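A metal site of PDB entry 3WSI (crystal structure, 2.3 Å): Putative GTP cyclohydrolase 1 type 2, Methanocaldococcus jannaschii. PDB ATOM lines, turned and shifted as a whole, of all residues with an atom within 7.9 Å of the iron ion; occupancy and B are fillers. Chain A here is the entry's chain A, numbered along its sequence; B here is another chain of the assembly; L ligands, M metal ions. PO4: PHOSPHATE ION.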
ATOM      1  N   LEU A  52      -5.013 -20.545 -31.394  1.00  0.00           N
ATOM      2  CA  LEU A  52      -4.532 -21.736 -30.713  1.00  0.00           C
ATOM      3  C   LEU A  52      -5.702 -22.378 -29.964  1.00  0.00           C
ATOM      4  O   LEU A  52      -6.007 -23.553 -30.156  1.00  0.00           O
ATOM      5  CB  LEU A  52      -3.395 -21.403 -29.764  1.00  0.00           C
ATOM      6  CG  LEU A  52      -2.759 -22.643 -29.112  1.00  0.00           C
ATOM      7  CD1 LEU A  52      -2.041 -23.501 -30.164  1.00  0.00           C
ATOM      8  CD2 LEU A  52      -1.841 -22.256 -27.985  1.00  0.00           C
ATOM      9  N   ASP A  53      -6.390 -21.577 -29.166  1.00  0.00           N
ATOM     10  CA  ASP A  53      -7.477 -22.045 -28.309  1.00  0.00           C
ATOM     11  C   ASP A  53      -8.836 -21.466 -28.700  1.00  0.00           C
ATOM     12  O   ASP A  53      -8.942 -20.261 -28.958  1.00  0.00           O
ATOM     13  CB  ASP A  53      -7.190 -21.687 -26.859  1.00  0.00           C
ATOM     14  CG  ASP A  53      -5.899 -22.276 -26.360  1.00  0.00           C
ATOM     15  OD1 ASP A  53      -5.749 -23.505 -26.461  1.00  0.00           O
ATOM     16  OD2 ASP A  53      -5.030 -21.508 -25.854  1.00  0.00           O
ATOM     17  N   HIS A  73      -6.622 -24.797 -33.257  1.00  0.00           N
ATOM     18  CA  HIS A  73      -5.817 -25.996 -33.172  1.00  0.00           C
ATOM     19  C   HIS A  73      -6.441 -26.956 -32.163  1.00  0.00           C
ATOM     20  O   HIS A  73      -6.555 -28.141 -32.422  1.00  0.00           O
ATOM     21  CB  HIS A  73      -4.373 -25.658 -32.761  1.00  0.00           C
ATOM     22  CG  HIS A  73      -3.492 -26.859 -32.581  1.00  0.00           C
ATOM     23  ND1 HIS A  73      -3.358 -27.833 -33.539  1.00  0.00           N
ATOM     24  CD2 HIS A  73      -2.746 -27.265 -31.536  1.00  0.00           C
ATOM     25  CE1 HIS A  73      -2.522 -28.768 -33.108  1.00  0.00           C
ATOM     26  NE2 HIS A  73      -2.131 -28.448 -31.895  1.00  0.00           N
ATOM     27  N   HIS A  74      -6.843 -26.430 -31.001  1.00  0.00           N
ATOM     28  CA  HIS A  74      -7.487 -27.249 -29.981  1.00  0.00           C
ATOM     29  C   HIS A  74      -8.976 -27.309 -30.201  1.00  0.00           C
ATOM     30  O   HIS A  74      -9.581 -26.293 -30.509  1.00  0.00           O
ATOM     31  CB  HIS A  74      -7.223 -26.709 -28.589  1.00  0.00           C
ATOM     32  CG  HIS A  74      -5.776 -26.691 -28.230  1.00  0.00           C
ATOM     33  ND1 HIS A  74      -5.082 -25.535 -27.940  1.00  0.00           N
ATOM     34  CD2 HIS A  74      -4.885 -27.706 -28.106  1.00  0.00           C
ATOM     35  CE1 HIS A  74      -3.830 -25.829 -27.661  1.00  0.00           C
ATOM     36  NE2 HIS A  74      -3.684 -27.138 -27.754  1.00  0.00           N
ATOM     37  N   PRO A  75      -9.573 -28.508 -30.026  1.00  0.00           N
ATOM     38  CA  PRO A  75     -11.027 -28.670 -30.123  1.00  0.00           C
ATOM     39  C   PRO A  75     -11.732 -27.838 -29.081  1.00  0.00           C
ATOM     40  O   PRO A  75     -11.137 -27.468 -28.056  1.00  0.00           O
ATOM     41  CB  PRO A  75     -11.238 -30.177 -29.857  1.00  0.00           C
ATOM     42  CG  PRO A  75      -9.919 -30.817 -30.184  1.00  0.00           C
ATOM     43  CD  PRO A  75      -8.867 -29.778 -29.809  1.00  0.00           C
ATOM     44  N   HIS A 106      -6.250 -30.716 -35.054  1.00  0.00           N
ATOM     45  CA  HIS A 106      -5.523 -30.887 -33.794  1.00  0.00           C
ATOM     46  C   HIS A 106      -4.300 -31.792 -34.029  1.00  0.00           C
ATOM     47  O   HIS A 106      -3.299 -31.316 -34.555  1.00  0.00           O
ATOM     48  CB  HIS A 106      -6.456 -31.437 -32.707  1.00  0.00           C
ATOM     49  CG  HIS A 106      -5.858 -31.480 -31.336  1.00  0.00           C
ATOM     50  ND1 HIS A 106      -6.237 -32.409 -30.379  1.00  0.00           N
ATOM     51  CD2 HIS A 106      -4.928 -30.699 -30.725  1.00  0.00           C
ATOM     52  CE1 HIS A 106      -5.550 -32.223 -29.275  1.00  0.00           C
ATOM     53  NE2 HIS A 106      -4.759 -31.182 -29.455  1.00  0.00           N
ATOM     54  N   ASP A 110      -0.541 -31.619 -35.891  1.00  0.00           N
ATOM     55  CA  ASP A 110       0.709 -31.932 -35.211  1.00  0.00           C
ATOM     56  C   ASP A 110       1.581 -32.871 -36.033  1.00  0.00           C
ATOM     57  O   ASP A 110       2.810 -32.758 -36.040  1.00  0.00           O
ATOM     58  CB  ASP A 110       0.436 -32.573 -33.846  1.00  0.00           C
ATOM     59  CG  ASP A 110      -0.166 -31.602 -32.836  1.00  0.00           C
ATOM     60  OD1 ASP A 110       0.236 -30.430 -32.790  1.00  0.00           O
ATOM     61  OD2 ASP A 110      -1.049 -32.038 -32.084  1.00  0.00           O
ATOM     62  N   LEU A 116       3.059 -28.957 -37.015  1.00  0.00           N
ATOM     63  CA  LEU A 116       3.641 -28.303 -35.843  1.00  0.00           C
ATOM     64  C   LEU A 116       4.937 -28.959 -35.370  1.00  0.00           C
ATOM     65  O   LEU A 116       5.905 -28.285 -34.997  1.00  0.00           O
ATOM     66  CB  LEU A 116       2.623 -28.276 -34.695  1.00  0.00           C
ATOM     67  CG  LEU A 116       1.280 -27.648 -35.080  1.00  0.00           C
ATOM     68  CD1 LEU A 116       0.503 -27.428 -33.823  1.00  0.00           C
ATOM     69  CD2 LEU A 116       1.467 -26.351 -35.871  1.00  0.00           C
ATOM     70  N   LEU A 179       8.419 -32.096 -29.156  1.00  0.00           N
ATOM     71  CA  LEU A 179       6.995 -32.394 -29.149  1.00  0.00           C
ATOM     72  C   LEU A 179       6.223 -31.113 -28.854  1.00  0.00           C
ATOM     73  O   LEU A 179       6.247 -30.632 -27.719  1.00  0.00           O
ATOM     74  CB  LEU A 179       6.678 -33.479 -28.111  1.00  0.00           C
ATOM     75  CG  LEU A 179       5.313 -34.192 -28.025  1.00  0.00           C
ATOM     76  CD1 LEU A 179       4.114 -33.257 -27.695  1.00  0.00           C
ATOM     77  CD2 LEU A 179       5.043 -34.948 -29.285  1.00  0.00           C
ATOM     78  N   SER A 180       5.519 -30.597 -29.863  1.00  0.00           N
ATOM     79  CA  SER A 180       4.777 -29.354 -29.704  1.00  0.00           C
ATOM     80  C   SER A 180       3.588 -29.528 -28.766  1.00  0.00           C
ATOM     81  O   SER A 180       2.770 -30.432 -28.941  1.00  0.00           O
ATOM     82  CB  SER A 180       4.290 -28.823 -31.046  1.00  0.00           C
ATOM     83  OG  SER A 180       3.560 -29.840 -31.695  1.00  0.00           O
ATOM     84  N   GLY A 181       3.481 -28.641 -27.796  1.00  0.00           N
ATOM     85  CA  GLY A 181       2.384 -28.689 -26.848  1.00  0.00           C
ATOM     86  C   GLY A 181       2.751 -29.374 -25.534  1.00  0.00           C
ATOM     87  O   GLY A 181       3.695 -28.969 -24.854  1.00  0.00           O
ATOM     88  N   TYR A 182       1.971 -30.379 -25.166  1.00  0.00           N
ATOM     89  CA  TYR A 182       2.174 -31.067 -23.906  1.00  0.00           C
ATOM     90  C   TYR A 182       2.740 -32.469 -24.141  1.00  0.00           C
ATOM     91  O   TYR A 182       2.011 -33.408 -24.481  1.00  0.00           O
ATOM     92  CB  TYR A 182       0.852 -31.118 -23.097  1.00  0.00           C
ATOM     93  CG  TYR A 182       0.916 -32.023 -21.892  1.00  0.00           C
ATOM     94  CD1 TYR A 182       1.957 -31.901 -20.968  1.00  0.00           C
ATOM     95  CD2 TYR A 182      -0.070 -32.994 -21.663  1.00  0.00           C
ATOM     96  CE1 TYR A 182       2.038 -32.732 -19.865  1.00  0.00           C
ATOM     97  CE2 TYR A 182      -0.006 -33.819 -20.547  1.00  0.00           C
ATOM     98  CZ  TYR A 182       1.055 -33.683 -19.640  1.00  0.00           C
ATOM     99  OH  TYR A 182       1.160 -34.488 -18.532  1.00  0.00           O
ATOM    100  N   ASP A 203       4.676 -27.499 -20.719  1.00  0.00           N
ATOM    101  CA  ASP A 203       3.802 -27.901 -19.597  1.00  0.00           C
ATOM    102  C   ASP A 203       4.503 -28.855 -18.613  1.00  0.00           C
ATOM    103  O   ASP A 203       3.961 -29.925 -18.264  1.00  0.00           O
ATOM    104  CB  ASP A 203       2.504 -28.563 -20.095  1.00  0.00           C
ATOM    105  CG  ASP A 203       1.355 -27.562 -20.337  1.00  0.00           C
ATOM    106  OD1 ASP A 203       1.455 -26.373 -19.938  1.00  0.00           O
ATOM    107  OD2 ASP A 203       0.323 -27.991 -20.894  1.00  0.00           O
ATOM    108  N   HIS A 224       3.810 -24.802 -23.455  1.00  0.00           N
ATOM    109  CA  HIS A 224       2.794 -25.374 -24.308  1.00  0.00           C
ATOM    110  C   HIS A 224       2.440 -24.415 -25.437  1.00  0.00           C
ATOM    111  O   HIS A 224       2.502 -24.777 -26.619  1.00  0.00           O
ATOM    112  CB  HIS A 224       1.567 -25.643 -23.432  1.00  0.00           C
ATOM    113  CG  HIS A 224       0.516 -26.477 -24.087  1.00  0.00           C
ATOM    114  ND1 HIS A 224      -0.119 -27.499 -23.430  1.00  0.00           N
ATOM    115  CD2 HIS A 224      -0.012 -26.440 -25.332  1.00  0.00           C
ATOM    116  CE1 HIS A 224      -0.985 -28.077 -24.245  1.00  0.00           C
ATOM    117  NE2 HIS A 224      -0.940 -27.449 -25.407  1.00  0.00           N
ATOM    118  N   TYR A 225       2.129 -23.181 -25.061  1.00  0.00           N
ATOM    119  CA  TYR A 225       1.744 -22.122 -25.992  1.00  0.00           C
ATOM    120  C   TYR A 225       2.798 -21.877 -27.068  1.00  0.00           C
ATOM    121  O   TYR A 225       2.508 -21.967 -28.259  1.00  0.00           O
ATOM    122  CB  TYR A 225       1.477 -20.819 -25.238  1.00  0.00           C
ATOM    123  CG  TYR A 225       1.159 -19.599 -26.099  1.00  0.00           C
ATOM    124  CD1 TYR A 225      -0.155 -19.319 -26.483  1.00  0.00           C
ATOM    125  CD2 TYR A 225       2.161 -18.712 -26.514  1.00  0.00           C
ATOM    126  CE1 TYR A 225      -0.463 -18.197 -27.235  1.00  0.00           C
ATOM    127  CE2 TYR A 225       1.865 -17.576 -27.286  1.00  0.00           C
ATOM    128  CZ  TYR A 225       0.543 -17.331 -27.643  1.00  0.00           C
ATOM    129  OH  TYR A 225       0.223 -16.243 -28.425  1.00  0.00           O
ATOM    130  N   THR A 227       5.568 -23.503 -28.035  1.00  0.00           N
ATOM    131  CA  THR A 227       6.035 -24.605 -28.882  1.00  0.00           C
ATOM    132  C   THR A 227       5.028 -24.995 -29.948  1.00  0.00           C
ATOM    133  O   THR A 227       5.385 -25.659 -30.925  1.00  0.00           O
ATOM    134  CB  THR A 227       6.408 -25.867 -28.075  1.00  0.00           C
ATOM    135  OG1 THR A 227       5.279 -26.298 -27.304  1.00  0.00           O
ATOM    136  CG2 THR A 227       7.638 -25.611 -27.153  1.00  0.00           C
ATOM    137  N   GLU A 228       3.774 -24.589 -29.768  1.00  0.00           N
ATOM    138  CA  GLU A 228       2.749 -24.791 -30.789  1.00  0.00           C
ATOM    139  C   GLU A 228       2.536 -23.592 -31.708  1.00  0.00           C
ATOM    140  O   GLU A 228       2.284 -23.764 -32.907  1.00  0.00           O
ATOM    141  CB  GLU A 228       1.444 -25.129 -30.136  1.00  0.00           C
ATOM    142  CG  GLU A 228       1.416 -26.549 -29.784  1.00  0.00           C
ATOM    143  CD  GLU A 228       0.172 -26.921 -29.059  1.00  0.00           C
ATOM    144  OE1 GLU A 228      -0.518 -26.013 -28.517  1.00  0.00           O
ATOM    145  OE2 GLU A 228      -0.118 -28.125 -29.090  1.00  0.00           O
ATOM    146  N   HIS B 206      -1.162 -25.152 -19.362  1.00  0.00           N
ATOM    147  CA  HIS B 206      -1.814 -24.228 -20.270  1.00  0.00           C
ATOM    148  C   HIS B 206      -3.363 -24.256 -20.299  1.00  0.00           C
ATOM    149  O   HIS B 206      -4.017 -23.201 -20.164  1.00  0.00           O
ATOM    150  CB  HIS B 206      -1.304 -24.475 -21.680  1.00  0.00           C
ATOM    151  CG  HIS B 206      -1.961 -23.598 -22.703  1.00  0.00           C
ATOM    152  ND1 HIS B 206      -1.760 -22.234 -22.766  1.00  0.00           N
ATOM    153  CD2 HIS B 206      -2.833 -23.892 -23.695  1.00  0.00           C
ATOM    154  CE1 HIS B 206      -2.485 -21.728 -23.737  1.00  0.00           C
ATOM    155  NE2 HIS B 206      -3.137 -22.723 -24.332  1.00  0.00           N
ATOM    156  N   HIS B 207      -3.975 -25.435 -20.488  1.00  0.00           N
ATOM    157  CA  HIS B 207      -5.441 -25.486 -20.620  1.00  0.00           C
ATOM    158  C   HIS B 207      -6.108 -24.999 -19.346  1.00  0.00           C
ATOM    159  O   HIS B 207      -7.142 -24.367 -19.405  1.00  0.00           O
ATOM    160  CB  HIS B 207      -5.950 -26.891 -20.986  1.00  0.00           C
ATOM    161  CG  HIS B 207      -5.591 -27.329 -22.373  1.00  0.00           C
ATOM    162  ND1 HIS B 207      -5.900 -26.575 -23.495  1.00  0.00           N
ATOM    163  CD2 HIS B 207      -4.951 -28.440 -22.829  1.00  0.00           C
ATOM    164  CE1 HIS B 207      -5.476 -27.207 -24.574  1.00  0.00           C
ATOM    165  NE2 HIS B 207      -4.906 -28.341 -24.207  1.00  0.00           N
HETATM  166  P   PO4 L   1      -2.714 -30.919 -26.393  1.00  0.00           P
HETATM  167  O1  PO4 L   1      -3.520 -30.190 -25.359  1.00  0.00           O
HETATM  168  O2  PO4 L   1      -2.444 -30.057 -27.600  1.00  0.00           O
HETATM  169  O3  PO4 L   1      -1.379 -31.304 -25.790  1.00  0.00           O
HETATM  170  O4  PO4 L   1      -3.434 -32.176 -26.839  1.00  0.00           O
HETATM  171 FE    FE M   1      -1.802 -28.173 -27.363  1.00  0.00          FE
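The iron ion is bound by an oxygen (O2) of the ligand (2.0 Å), a ring nitrogen (NE2) of His 74 (2.2 Å), a ring nitrogen (NE2) of His 224 (2.3 Å) and the side-chain carboxylate of Glu 228 (2.4 Å).
Slightly farther from the iron ion lies the side-chain carboxylate (OE1) of Glu 228 (2.8 Å).
The side-chain carboxylate (OE2) of Glu 228 lies close to a ring nitrogen (NE2) of His 73, at 3.5 Å.
ND1 of His 224 lies within hydrogen-bond range of OD2 of Asp 203, 2.6 Å away.
The side-chain hydroxyl (OG1) of Thr 227 lies within hydrogen-bond range of the backbone carbonyl oxygen (O) of His 224.
The backbone carbonyl oxygen (O) of Leu 52 sits at hydrogen-bond distance from the backbone NH (N) of His 74 (3.1 Å).
A ring nitrogen (ND1) of His 74 is in hydrogen-bond range of the side-chain carboxylate (OD1) of Asp 53 (2.6 Å).
The nearest printed residue that does not touch the iron ion is Gly 181 (4.2 Å).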
